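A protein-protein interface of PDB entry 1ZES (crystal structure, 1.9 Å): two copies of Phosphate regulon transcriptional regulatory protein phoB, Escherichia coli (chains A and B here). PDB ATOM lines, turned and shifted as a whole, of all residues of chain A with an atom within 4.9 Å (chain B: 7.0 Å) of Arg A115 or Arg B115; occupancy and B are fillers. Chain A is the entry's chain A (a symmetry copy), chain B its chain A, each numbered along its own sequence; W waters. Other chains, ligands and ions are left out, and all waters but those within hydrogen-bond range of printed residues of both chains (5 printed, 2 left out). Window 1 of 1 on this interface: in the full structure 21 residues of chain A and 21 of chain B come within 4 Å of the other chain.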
ATOM      1  N   LEU A  95     -13.547  14.965  -7.910  1.00  0.00           N
ATOM      2  CA  LEU A  95     -12.270  15.156  -8.585  1.00  0.00           C
ATOM      3  C   LEU A  95     -11.091  14.554  -7.821  1.00  0.00           C
ATOM      4  O   LEU A  95     -10.253  13.881  -8.407  1.00  0.00           O
ATOM      5  CB  LEU A  95     -12.042  16.648  -8.840  1.00  0.00           C
ATOM      6  CG  LEU A  95     -13.024  17.205  -9.902  1.00  0.00           C
ATOM      7  CD1 LEU A  95     -13.101  18.736  -9.685  1.00  0.00           C
ATOM      8  CD2 LEU A  95     -12.590  16.850 -11.334  1.00  0.00           C
ATOM      9  N   ASP A 101     -13.412  14.555 -14.660  1.00  0.00           N
ATOM     10  CA  ASP A 101     -14.294  15.730 -14.748  1.00  0.00           C
ATOM     11  C   ASP A 101     -15.535  15.445 -13.918  1.00  0.00           C
ATOM     12  O   ASP A 101     -15.786  14.298 -13.528  1.00  0.00           O
ATOM     13  CB  ASP A 101     -14.667  16.020 -16.224  1.00  0.00           C
ATOM     14  CG  ASP A 101     -15.021  17.488 -16.499  1.00  0.00           C
ATOM     15  OD1 ASP A 101     -15.456  18.223 -15.582  1.00  0.00           O
ATOM     16  OD2 ASP A 101     -14.914  17.897 -17.700  1.00  0.00           O
ATOM     17  N   TYR A 102     -16.318  16.487 -13.673  1.00  0.00           N
ATOM     18  CA  TYR A 102     -17.446  16.428 -12.768  1.00  0.00           C
ATOM     19  C   TYR A 102     -18.474  17.417 -13.288  1.00  0.00           C
ATOM     20  O   TYR A 102     -18.224  18.640 -13.302  1.00  0.00           O
ATOM     21  CB  TYR A 102     -16.957  16.806 -11.358  1.00  0.00           C
ATOM     22  CG  TYR A 102     -17.952  16.615 -10.232  1.00  0.00           C
ATOM     23  CD1 TYR A 102     -19.078  17.428 -10.131  1.00  0.00           C
ATOM     24  CD2 TYR A 102     -17.765  15.615  -9.277  1.00  0.00           C
ATOM     25  CE1 TYR A 102     -19.991  17.267  -9.090  1.00  0.00           C
ATOM     26  CE2 TYR A 102     -18.706  15.441  -8.214  1.00  0.00           C
ATOM     27  CZ  TYR A 102     -19.810  16.278  -8.157  1.00  0.00           C
ATOM     28  OH  TYR A 102     -20.727  16.162  -7.120  1.00  0.00           O
ATOM     29  N   ILE A 103     -19.604  16.900 -13.767  1.00  0.00           N
ATOM     30  CA  ILE A 103     -20.657  17.751 -14.362  1.00  0.00           C
ATOM     31  C   ILE A 103     -21.930  17.663 -13.541  1.00  0.00           C
ATOM     32  O   ILE A 103     -22.306  16.566 -13.085  1.00  0.00           O
ATOM     33  CB  ILE A 103     -20.960  17.342 -15.832  1.00  0.00           C
ATOM     34  CG1 ILE A 103     -19.668  17.368 -16.656  1.00  0.00           C
ATOM     35  CG2 ILE A 103     -21.991  18.298 -16.475  1.00  0.00           C
ATOM     36  CD1 ILE A 103     -19.812  16.589 -18.022  1.00  0.00           C
ATOM     37  N   GLU A 111     -22.303  20.606 -23.797  1.00  0.00           N
ATOM     38  CA  GLU A 111     -21.209  20.613 -22.853  1.00  0.00           C
ATOM     39  C   GLU A 111     -20.873  19.204 -22.365  1.00  0.00           C
ATOM     40  O   GLU A 111     -19.696  18.847 -22.184  1.00  0.00           O
ATOM     41  CB  GLU A 111     -21.504  21.560 -21.676  1.00  0.00           C
ATOM     42  CG  GLU A 111     -20.301  21.639 -20.728  1.00  0.00           C
ATOM     43  CD  GLU A 111     -20.531  22.566 -19.561  1.00  0.00           C
ATOM     44  OE1 GLU A 111     -21.697  22.925 -19.278  1.00  0.00           O
ATOM     45  OE2 GLU A 111     -19.521  22.944 -18.944  1.00  0.00           O
ATOM     46  N   LEU A 112     -21.882  18.365 -22.181  1.00  0.00           N
ATOM     47  CA  LEU A 112     -21.604  16.980 -21.729  1.00  0.00           C
ATOM     48  C   LEU A 112     -20.704  16.272 -22.736  1.00  0.00           C
ATOM     49  O   LEU A 112     -19.626  15.753 -22.402  1.00  0.00           O
ATOM     50  CB  LEU A 112     -22.926  16.200 -21.487  1.00  0.00           C
ATOM     51  CG  LEU A 112     -22.747  14.682 -21.316  1.00  0.00           C
ATOM     52  CD1 LEU A 112     -21.864  14.338 -20.074  1.00  0.00           C
ATOM     53  CD2 LEU A 112     -24.095  13.946 -21.252  1.00  0.00           C
ATOM     54  N   VAL A 113     -21.124  16.297 -23.996  1.00  0.00           N
ATOM     55  CA  VAL A 113     -20.356  15.681 -25.068  1.00  0.00           C
ATOM     56  C   VAL A 113     -18.953  16.323 -25.238  1.00  0.00           C
ATOM     57  O   VAL A 113     -17.959  15.611 -25.444  1.00  0.00           O
ATOM     58  CB  VAL A 113     -21.186  15.655 -26.369  1.00  0.00           C
ATOM     59  CG1 VAL A 113     -20.342  15.312 -27.557  1.00  0.00           C
ATOM     60  CG2 VAL A 113     -22.418  14.674 -26.218  1.00  0.00           C
ATOM     61  N   ALA A 114     -18.876  17.660 -25.145  1.00  0.00           N
ATOM     62  CA  ALA A 114     -17.606  18.381 -25.266  1.00  0.00           C
ATOM     63  C   ALA A 114     -16.588  17.968 -24.203  1.00  0.00           C
ATOM     64  O   ALA A 114     -15.373  17.841 -24.493  1.00  0.00           O
ATOM     65  CB  ALA A 114     -17.863  19.906 -25.193  1.00  0.00           C
ATOM     66  N   ARG A 115     -17.066  17.838 -22.954  1.00  0.00           N
ATOM     67  CA  ARG A 115     -16.210  17.364 -21.855  1.00  0.00           C
ATOM     68  C   ARG A 115     -15.793  15.922 -22.021  1.00  0.00           C
ATOM     69  O   ARG A 115     -14.618  15.574 -21.789  1.00  0.00           O
ATOM     70  CB  ARG A 115     -16.864  17.648 -20.505  1.00  0.00           C
ATOM     71  CG  ARG A 115     -17.066  19.152 -20.251  1.00  0.00           C
ATOM     72  CD  ARG A 115     -17.694  19.475 -18.858  1.00  0.00           C
ATOM     73  NE  ARG A 115     -17.565  20.889 -18.580  1.00  0.00           N
ATOM     74  CZ  ARG A 115     -16.476  21.464 -18.087  1.00  0.00           C
ATOM     75  NH1 ARG A 115     -15.432  20.730 -17.752  1.00  0.00           N
ATOM     76  NH2 ARG A 115     -16.442  22.783 -17.894  1.00  0.00           N
ATOM     77  N   ILE A 116     -16.716  15.055 -22.444  1.00  0.00           N
ATOM     78  CA  ILE A 116     -16.335  13.651 -22.675  1.00  0.00           C
ATOM     79  C   ILE A 116     -15.251  13.588 -23.761  1.00  0.00           C
ATOM     80  O   ILE A 116     -14.232  12.904 -23.607  1.00  0.00           O
ATOM     81  CB  ILE A 116     -17.569  12.808 -23.073  1.00  0.00           C
ATOM     82  CG1 ILE A 116     -18.463  12.605 -21.835  1.00  0.00           C
ATOM     83  CG2 ILE A 116     -17.151  11.509 -23.782  1.00  0.00           C
ATOM     84  CD1 ILE A 116     -19.846  12.046 -22.177  1.00  0.00           C
ATOM     85  N   LYS A 117     -15.463  14.300 -24.870  1.00  0.00           N
ATOM     86  CA  LYS A 117     -14.466  14.256 -25.943  1.00  0.00           C
ATOM     87  C   LYS A 117     -13.132  14.910 -25.510  1.00  0.00           C
ATOM     88  O   LYS A 117     -12.075  14.412 -25.869  1.00  0.00           O
ATOM     89  CB  LYS A 117     -14.998  14.826 -27.255  1.00  0.00           C
ATOM     90  CG  LYS A 117     -16.145  13.994 -27.820  1.00  0.00           C
ATOM     91  CD  LYS A 117     -16.813  14.656 -28.983  1.00  0.00           C
ATOM     92  CE  LYS A 117     -17.755  13.648 -29.675  1.00  0.00           C
ATOM     93  NZ  LYS A 117     -18.094  14.014 -31.089  1.00  0.00           N
ATOM     94  N   ALA A 118     -13.184  15.970 -24.708  1.00  0.00           N
ATOM     95  CA  ALA A 118     -11.948  16.564 -24.161  1.00  0.00           C
ATOM     96  C   ALA A 118     -11.145  15.545 -23.358  1.00  0.00           C
ATOM     97  O   ALA A 118      -9.923  15.353 -23.556  1.00  0.00           O
ATOM     98  CB  ALA A 118     -12.281  17.780 -23.306  1.00  0.00           C
ATOM     99  N   VAL A 119     -11.838  14.840 -22.474  1.00  0.00           N
ATOM    100  CA  VAL A 119     -11.212  13.786 -21.698  1.00  0.00           C
ATOM    101  C   VAL A 119     -10.644  12.686 -22.623  1.00  0.00           C
ATOM    102  O   VAL A 119      -9.483  12.279 -22.486  1.00  0.00           O
ATOM    103  CB  VAL A 119     -12.204  13.237 -20.645  1.00  0.00           C
ATOM    104  CG1 VAL A 119     -11.617  12.018 -19.922  1.00  0.00           C
ATOM    105  CG2 VAL A 119     -12.570  14.339 -19.645  1.00  0.00           C
ATOM    106  N   LEU B  49       1.263  22.819 -18.043  1.00  0.00           N
ATOM    107  CA  LEU B  49      -0.123  23.207 -18.325  1.00  0.00           C
ATOM    108  C   LEU B  49      -0.223  24.720 -18.423  1.00  0.00           C
ATOM    109  O   LEU B  49       0.540  25.454 -17.810  1.00  0.00           O
ATOM    110  CB  LEU B  49      -1.063  22.688 -17.231  1.00  0.00           C
ATOM    111  CG  LEU B  49      -2.592  22.809 -17.250  1.00  0.00           C
ATOM    112  CD1 LEU B  49      -3.222  21.529 -16.631  1.00  0.00           C
ATOM    113  CD2 LEU B  49      -3.036  24.049 -16.514  1.00  0.00           C
ATOM    114  N   VAL B  80      -6.374  24.683 -19.527  1.00  0.00           N
ATOM    115  CA  VAL B  80      -7.572  24.821 -18.713  1.00  0.00           C
ATOM    116  C   VAL B  80      -7.977  26.294 -18.767  1.00  0.00           C
ATOM    117  O   VAL B  80      -7.190  27.160 -18.386  1.00  0.00           O
ATOM    118  CB  VAL B  80      -7.256  24.422 -17.279  1.00  0.00           C
ATOM    119  CG1 VAL B  80      -8.401  24.830 -16.350  1.00  0.00           C
ATOM    120  CG2 VAL B  80      -6.975  22.875 -17.209  1.00  0.00           C
ATOM    121  N   ARG B  91     -18.555  28.096 -22.625  1.00  0.00           N
ATOM    122  CA  ARG B  91     -18.004  26.846 -22.103  1.00  0.00           C
ATOM    123  C   ARG B  91     -17.832  25.843 -23.216  1.00  0.00           C
ATOM    124  O   ARG B  91     -16.756  25.379 -23.411  1.00  0.00           O
ATOM    125  CB  ARG B  91     -18.871  26.288 -20.982  1.00  0.00           C
ATOM    126  CG  ARG B  91     -19.183  27.351 -19.938  1.00  0.00           C
ATOM    127  CD  ARG B  91     -19.595  26.725 -18.629  1.00  0.00           C
ATOM    128  NE  ARG B  91     -20.761  25.848 -18.741  1.00  0.00           N
ATOM    129  CZ  ARG B  91     -22.013  26.226 -18.494  1.00  0.00           C
ATOM    130  NH1 ARG B  91     -22.279  27.472 -18.139  1.00  0.00           N
ATOM    131  NH2 ARG B  91     -23.010  25.350 -18.630  1.00  0.00           N
ATOM    132  N   LEU B  95     -14.105  24.436 -24.807  1.00  0.00           N
ATOM    133  CA  LEU B  95     -13.839  23.005 -24.878  1.00  0.00           C
ATOM    134  C   LEU B  95     -13.642  22.501 -26.307  1.00  0.00           C
ATOM    135  O   LEU B  95     -12.711  21.752 -26.577  1.00  0.00           O
ATOM    136  CB  LEU B  95     -14.970  22.238 -24.188  1.00  0.00           C
ATOM    137  CG  LEU B  95     -14.962  22.464 -22.653  1.00  0.00           C
ATOM    138  CD1 LEU B  95     -16.388  22.141 -22.145  1.00  0.00           C
ATOM    139  CD2 LEU B  95     -13.894  21.612 -21.949  1.00  0.00           C
ATOM    140  N   ALA B  99      -9.622  23.150 -25.307  1.00  0.00           N
ATOM    141  CA  ALA B  99      -9.416  23.250 -23.850  1.00  0.00           C
ATOM    142  C   ALA B  99      -9.719  21.899 -23.219  1.00  0.00           C
ATOM    143  O   ALA B  99     -10.679  21.218 -23.594  1.00  0.00           O
ATOM    144  CB  ALA B  99     -10.303  24.321 -23.226  1.00  0.00           C
ATOM    145  N   ASP B 100      -8.866  21.485 -22.302  1.00  0.00           N
ATOM    146  CA  ASP B 100      -9.091  20.241 -21.570  1.00  0.00           C
ATOM    147  C   ASP B 100     -10.114  20.423 -20.443  1.00  0.00           C
ATOM    148  O   ASP B 100     -10.758  19.464 -20.020  1.00  0.00           O
ATOM    149  CB  ASP B 100      -7.746  19.757 -21.069  1.00  0.00           C
ATOM    150  CG  ASP B 100      -6.775  19.517 -22.222  1.00  0.00           C
ATOM    151  OD1 ASP B 100      -6.870  18.441 -22.830  1.00  0.00           O
ATOM    152  OD2 ASP B 100      -5.960  20.404 -22.544  1.00  0.00           O
ATOM    153  N   ASP B 101     -10.274  21.658 -19.976  1.00  0.00           N
ATOM    154  CA  ASP B 101     -11.289  22.009 -18.970  1.00  0.00           C
ATOM    155  C   ASP B 101     -11.552  23.502 -19.072  1.00  0.00           C
ATOM    156  O   ASP B 101     -10.788  24.237 -19.711  1.00  0.00           O
ATOM    157  CB  ASP B 101     -10.801  21.626 -17.549  1.00  0.00           C
ATOM    158  CG  ASP B 101     -11.939  21.356 -16.553  1.00  0.00           C
ATOM    159  OD1 ASP B 101     -13.067  21.878 -16.715  1.00  0.00           O
ATOM    160  OD2 ASP B 101     -11.664  20.641 -15.536  1.00  0.00           O
ATOM    161  N   TYR B 102     -12.620  23.947 -18.424  1.00  0.00           N
ATOM    162  CA  TYR B 102     -13.107  25.304 -18.547  1.00  0.00           C
ATOM    163  C   TYR B 102     -13.751  25.658 -17.218  1.00  0.00           C
ATOM    164  O   TYR B 102     -14.774  25.057 -16.831  1.00  0.00           O
ATOM    165  CB  TYR B 102     -14.125  25.351 -19.702  1.00  0.00           C
ATOM    166  CG  TYR B 102     -14.604  26.726 -20.115  1.00  0.00           C
ATOM    167  CD1 TYR B 102     -15.423  27.476 -19.275  1.00  0.00           C
ATOM    168  CD2 TYR B 102     -14.228  27.275 -21.342  1.00  0.00           C
ATOM    169  CE1 TYR B 102     -15.879  28.739 -19.654  1.00  0.00           C
ATOM    170  CE2 TYR B 102     -14.686  28.573 -21.729  1.00  0.00           C
ATOM    171  CZ  TYR B 102     -15.502  29.278 -20.857  1.00  0.00           C
ATOM    172  OH  TYR B 102     -15.995  30.528 -21.213  1.00  0.00           O
ATOM    173  N   ILE B 103     -13.136  26.589 -16.492  1.00  0.00           N
ATOM    174  CA  ILE B 103     -13.625  26.977 -15.152  1.00  0.00           C
ATOM    175  C   ILE B 103     -14.053  28.433 -15.149  1.00  0.00           C
ATOM    176  O   ILE B 103     -13.374  29.286 -15.752  1.00  0.00           O
ATOM    177  CB  ILE B 103     -12.538  26.756 -14.059  1.00  0.00           C
ATOM    178  CG1 ILE B 103     -12.054  25.304 -14.095  1.00  0.00           C
ATOM    179  CG2 ILE B 103     -13.091  27.073 -12.651  1.00  0.00           C
ATOM    180  CD1 ILE B 103     -10.694  25.105 -13.316  1.00  0.00           C
ATOM    181  N   THR B 104     -15.179  28.728 -14.491  1.00  0.00           N
ATOM    182  CA  THR B 104     -15.742  30.088 -14.539  1.00  0.00           C
ATOM    183  C   THR B 104     -15.363  30.854 -13.273  1.00  0.00           C
ATOM    184  O   THR B 104     -15.257  30.252 -12.206  1.00  0.00           O
ATOM    185  CB  THR B 104     -17.272  30.045 -14.599  1.00  0.00           C
ATOM    186  OG1 THR B 104     -17.732  29.225 -13.518  1.00  0.00           O
ATOM    187  CG2 THR B 104     -17.758  29.429 -15.873  1.00  0.00           C
ATOM    188  N   LYS B 110      -9.817  25.353  -4.213  1.00  0.00           N
ATOM    189  CA  LYS B 110      -9.785  23.872  -4.140  1.00  0.00           C
ATOM    190  C   LYS B 110     -10.220  23.147  -5.431  1.00  0.00           C
ATOM    191  O   LYS B 110      -9.584  22.164  -5.857  1.00  0.00           O
ATOM    192  CB  LYS B 110     -10.678  23.399  -2.986  1.00  0.00           C
ATOM    193  CG  LYS B 110     -10.212  23.836  -1.590  1.00  0.00           C
ATOM    194  CD  LYS B 110     -11.392  23.778  -0.581  1.00  0.00           C
ATOM    195  CE  LYS B 110     -12.077  22.376  -0.555  1.00  0.00           C
ATOM    196  NZ  LYS B 110     -13.578  22.442  -0.247  1.00  0.00           N
ATOM    197  N   GLU B 111     -11.319  23.592  -6.035  1.00  0.00           N
ATOM    198  CA  GLU B 111     -11.740  23.044  -7.305  1.00  0.00           C
ATOM    199  C   GLU B 111     -10.764  23.399  -8.427  1.00  0.00           C
ATOM    200  O   GLU B 111     -10.477  22.579  -9.316  1.00  0.00           O
ATOM    201  CB  GLU B 111     -13.174  23.487  -7.645  1.00  0.00           C
ATOM    202  CG  GLU B 111     -13.652  22.825  -8.944  1.00  0.00           C
ATOM    203  CD  GLU B 111     -15.059  23.213  -9.318  1.00  0.00           C
ATOM    204  OE1 GLU B 111     -15.587  24.216  -8.784  1.00  0.00           O
ATOM    205  OE2 GLU B 111     -15.636  22.488 -10.147  1.00  0.00           O
ATOM    206  N   LEU B 112     -10.206  24.601  -8.392  1.00  0.00           N
ATOM    207  CA  LEU B 112      -9.236  24.982  -9.448  1.00  0.00           C
ATOM    208  C   LEU B 112      -8.055  24.019  -9.447  1.00  0.00           C
ATOM    209  O   LEU B 112      -7.714  23.397 -10.467  1.00  0.00           O
ATOM    210  CB  LEU B 112      -8.778  26.457  -9.271  1.00  0.00           C
ATOM    211  CG  LEU B 112      -7.557  26.850 -10.120  1.00  0.00           C
ATOM    212  CD1 LEU B 112      -7.846  26.716 -11.650  1.00  0.00           C
ATOM    213  CD2 LEU B 112      -7.047  28.259  -9.778  1.00  0.00           C
ATOM    214  N   VAL B 113      -7.455  23.849  -8.273  1.00  0.00           N
ATOM    215  CA  VAL B 113      -6.327  22.942  -8.118  1.00  0.00           C
ATOM    216  C   VAL B 113      -6.699  21.471  -8.446  1.00  0.00           C
ATOM    217  O   VAL B 113      -5.921  20.758  -9.097  1.00  0.00           O
ATOM    218  CB  VAL B 113      -5.690  23.122  -6.725  1.00  0.00           C
ATOM    219  CG1 VAL B 113      -4.731  22.016  -6.407  1.00  0.00           C
ATOM    220  CG2 VAL B 113      -5.008  24.545  -6.609  1.00  0.00           C
ATOM    221  N   ALA B 114      -7.885  21.026  -8.003  1.00  0.00           N
ATOM    222  CA  ALA B 114      -8.358  19.664  -8.267  1.00  0.00           C
ATOM    223  C   ALA B 114      -8.486  19.361  -9.760  1.00  0.00           C
ATOM    224  O   ALA B 114      -8.151  18.243 -10.221  1.00  0.00           O
ATOM    225  CB  ALA B 114      -9.717  19.437  -7.560  1.00  0.00           C
ATOM    226  N   ARG B 115      -9.049  20.328 -10.506  1.00  0.00           N
ATOM    227  CA  ARG B 115      -9.153  20.197 -11.968  1.00  0.00           C
ATOM    228  C   ARG B 115      -7.808  20.223 -12.654  1.00  0.00           C
ATOM    229  O   ARG B 115      -7.555  19.424 -13.576  1.00  0.00           O
ATOM    230  CB  ARG B 115     -10.133  21.226 -12.529  1.00  0.00           C
ATOM    231  CG  ARG B 115     -11.563  21.034 -11.993  1.00  0.00           C
ATOM    232  CD  ARG B 115     -12.596  22.045 -12.584  1.00  0.00           C
ATOM    233  NE  ARG B 115     -13.940  21.608 -12.275  1.00  0.00           N
ATOM    234  CZ  ARG B 115     -14.615  20.700 -12.969  1.00  0.00           C
ATOM    235  NH1 ARG B 115     -14.092  20.176 -14.060  1.00  0.00           N
ATOM    236  NH2 ARG B 115     -15.840  20.339 -12.585  1.00  0.00           N
ATOM    237  N   ILE B 116      -6.908  21.109 -12.221  1.00  0.00           N
ATOM    238  CA  ILE B 116      -5.565  21.128 -12.823  1.00  0.00           C
ATOM    239  C   ILE B 116      -4.883  19.771 -12.590  1.00  0.00           C
ATOM    240  O   ILE B 116      -4.311  19.178 -13.514  1.00  0.00           O
ATOM    241  CB  ILE B 116      -4.718  22.282 -12.238  1.00  0.00           C
ATOM    242  CG1 ILE B 116      -5.239  23.622 -12.791  1.00  0.00           C
ATOM    243  CG2 ILE B 116      -3.216  22.038 -12.457  1.00  0.00           C
ATOM    244  CD1 ILE B 116      -4.674  24.838 -12.054  1.00  0.00           C
ATOM    245  N   LYS B 117      -4.935  19.271 -11.355  1.00  0.00           N
ATOM    246  CA  LYS B 117      -4.281  17.989 -11.079  1.00  0.00           C
ATOM    247  C   LYS B 117      -4.977  16.823 -11.820  1.00  0.00           C
ATOM    248  O   LYS B 117      -4.300  15.926 -12.300  1.00  0.00           O
ATOM    249  CB  LYS B 117      -4.128  17.723  -9.585  1.00  0.00           C
ATOM    250  CG  LYS B 117      -3.199  18.731  -8.914  1.00  0.00           C
ATOM    251  CD  LYS B 117      -3.210  18.615  -7.423  1.00  0.00           C
ATOM    252  CE  LYS B 117      -2.053  19.449  -6.836  1.00  0.00           C
ATOM    253  NZ  LYS B 117      -1.659  19.040  -5.446  1.00  0.00           N
ATOM    254  N   ALA B 118      -6.300  16.867 -11.957  1.00  0.00           N
ATOM    255  CA  ALA B 118      -7.009  15.850 -12.759  1.00  0.00           C
ATOM    256  C   ALA B 118      -6.500  15.814 -14.197  1.00  0.00           C
ATOM    257  O   ALA B 118      -6.156  14.747 -14.756  1.00  0.00           O
ATOM    258  CB  ALA B 118      -8.511  16.108 -12.728  1.00  0.00           C
ATOM    259  N   VAL B 119      -6.396  16.993 -14.796  1.00  0.00           N
ATOM    260  CA  VAL B 119      -5.853  17.108 -16.136  1.00  0.00           C
ATOM    261  C   VAL B 119      -4.401  16.585 -16.189  1.00  0.00           C
ATOM    262  O   VAL B 119      -4.049  15.776 -17.057  1.00  0.00           O
ATOM    263  CB  VAL B 119      -5.990  18.564 -16.644  1.00  0.00           C
ATOM    264  CG1 VAL B 119      -5.283  18.742 -17.994  1.00  0.00           C
ATOM    265  CG2 VAL B 119      -7.470  18.945 -16.752  1.00  0.00           C
ATOM    266  N   MET B 120      -3.563  17.031 -15.261  1.00  0.00           N
ATOM    267  CA  MET B 120      -2.168  16.562 -15.159  1.00  0.00           C
ATOM    268  C   MET B 120      -2.027  15.040 -14.980  1.00  0.00           C
ATOM    269  O   MET B 120      -1.032  14.468 -15.400  1.00  0.00           O
ATOM    270  CB  MET B 120      -1.438  17.273 -13.999  1.00  0.00           C
ATOM    271  CG  MET B 120      -1.528  18.801 -13.993  1.00  0.00           C
ATOM    272  SD  MET B 120       0.020  19.695 -14.145  1.00  0.00           S
ATOM    273  CE  MET B 120       0.315  19.242 -15.847  1.00  0.00           C
ATOM    274  N   ARG B 121      -3.000  14.400 -14.328  1.00  0.00           N
ATOM    275  CA  ARG B 121      -3.019  12.930 -14.173  1.00  0.00           C
ATOM    276  C   ARG B 121      -3.214  12.240 -15.526  1.00  0.00           C
ATOM    277  O   ARG B 121      -2.689  11.154 -15.752  1.00  0.00           O
ATOM    278  CB  ARG B 121      -4.118  12.454 -13.187  1.00  0.00           C
ATOM    279  CG  ARG B 121      -3.923  12.847 -11.711  1.00  0.00           C
ATOM    280  CD  ARG B 121      -4.867  12.057 -10.764  1.00  0.00           C
ATOM    281  NE  ARG B 121      -6.303  12.200 -11.086  1.00  0.00           N
ATOM    282  CZ  ARG B 121      -7.153  13.017 -10.453  1.00  0.00           C
ATOM    283  NH1 ARG B 121      -6.737  13.774  -9.432  1.00  0.00           N
ATOM    284  NH2 ARG B 121      -8.433  13.067 -10.826  1.00  0.00           N
HETATM  285  O   HOH W   1     -15.390  22.870 -14.937  1.00  0.00           O
HETATM  286  O   HOH W   2      -8.295  18.118 -24.920  1.00  0.00           O
HETATM  287  O   HOH W   3     -17.368  20.634 -15.311  1.00  0.00           O
HETATM  288  O   HOH W   4      -7.821  16.188  -8.664  1.00  0.00           O
HETATM  289  O   HOH W   5     -14.395  18.845 -26.681  1.00  0.00           O
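NH2 of Arg B91 lies within salt-bridge range of OE1 of Glu A111, 2.8 Å away.
The guanidinium group of Arg A115 lies within salt-bridge range of the side-chain carboxylate of Asp B101 (2.8 Å).
The guanidinium group (NH2) of Arg A115 lies within hydrogen-bond range of the backbone carbonyl oxygen (O) of Tyr B102, 3.0 Å away.
The side-chain carboxylate (OD1) of Asp A101 lies within salt-bridge range of the guanidinium group (NH1) of Arg B115 (2.8 Å).
O of Tyr A102 lies within hydrogen-bond range of NH2 of Arg B115 (3.0 Å).
The guanidinium group of Arg B121 sits at hydrogen-bond distance from the backbone carbonyl oxygen of Leu A95 (3.1 Å).
The side-chain carboxylate of Asp B101 lies within salt-bridge range of the guanidinium group of Arg B115.
The guanidinium group of Arg B115 is in salt-bridge range of the side-chain carboxylate of Glu B111 (2.9 Å).
The side-chain carboxylate (OD2) of Asp A101 lies within salt-bridge range of the guanidinium group (NH1) of Arg A115.
The side-chain carboxylate (OE2) of Glu A111 lies within salt-bridge range of the guanidinium group (NE) of Arg A115.
Among the printed residues, merely in contact across the chains: Leu A95 with Arg B115 (3.6 Å), Arg A115 with Leu B95 (3.6 Å), Ala A118 with Ala B99 (3.8 Å), Ala A114 with Leu B95 (3.8 Å), Leu A95 with Ala B114 (3.9 Å), Arg A115 with Arg B115 (3.97 Å) and Ala A118 with Asp B100 (3.99 Å).
Printed residues of chain B within 4 Å of Arg A115: Leu B95 (3.6 Å), Asp B101 (2.8 Å), Tyr B102 (3.0 Å) and Arg B115 (3.97 Å).
Of chain A, only Leu A95 (3.6 Å), Asp A101 (2.8 Å), Tyr A102 (3.0 Å) and Arg A115 (3.97 Å) come within 4 Å of Arg B115.
Printed residues of chain B within 4 Å of Leu A95: Ala B114 (3.9 Å), Arg B115 (3.6 Å) and Arg B121 (3.1 Å).
Printed residues of chain A within 4 Å of Asp B100: Ala A118.
Of the printed residues of chain A, Asp B101 touches Arg A115.
Of the printed residues of chain B, Ala A114 touches Leu B95 (3.8 Å).
Ala B118 touches none of the printed residues of chain A.
The nearest printed residue of chain A that does not touch Arg B115 is Ile A103 (5.2 Å).
Of the 13 printed residues of chain A, 7 touch a printed residue of chain B.
Hydrophobic or aromatic side chains of chain A within 4 Å of the printed part of chain B: Leu A95, Tyr A102, Ala A114 and Ala A118.
Hydrophobic or aromatic side chains of chain B within 4 Å of the printed part of chain A: Leu B95, Tyr B102 and Ala B114.
Along chain B the printed residues that touch a printed residue of chain A span positions 91 to 121.
Among the printed residues, Asp or Glu carboxylates within 4 Å of a Lys or Arg side-chain nitrogen of the other chain: Asp A101 with Arg B115, Glu A111 with Arg B91 and Arg A115 with Asp B101.
Leu A95 touches Ala B114, and with the chains exchanged Ala A114 touches Leu B95.
Leu A95 touches Arg B115, and with the chains exchanged Arg A115 touches Leu B95.
Asp A101 touches Arg B115, and with the chains exchanged Arg A115 touches Asp B101.
Arg A115 touches its own counterpart, Arg B115.
Positions printed for both chains: 95, 101, 102, 103, 111, 112, 113, 114, 115, 116, 117, 118 and 119.
Of the 13 pairs that touch across the chains among the printed residues, 9 have their exchanged pair printed and touching as well.
Water W2 lies within hydrogen-bond range of the side-chain carboxylate of Asp B100 (2.6 Å) and the backbone carbonyl oxygen of Ala A118 (3.5 Å).
Water W5 bridges O of Ala A114 (2.6 Å) and O of Leu B95 (3.4 Å).
Water W4 lies within hydrogen-bond range of the backbone carbonyl oxygen of Ala B114, the guanidinium group of Arg B121 and the backbone carbonyl oxygen of Leu A95.
Water W1 lies within hydrogen-bond range of O of Tyr B102 (3.0 Å), OD1 of Asp B101 (3.1 Å), NH1 of Arg B115 (3.1 Å) and NH2 of Arg A115 (3.1 Å).
Water W3 lies within hydrogen-bond range of O of Tyr A102 (3.0 Å), OD1 of Asp A101 (3.1 Å), NH1 of Arg A115 (3.1 Å) and NH2 of Arg B115 (3.1 Å).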
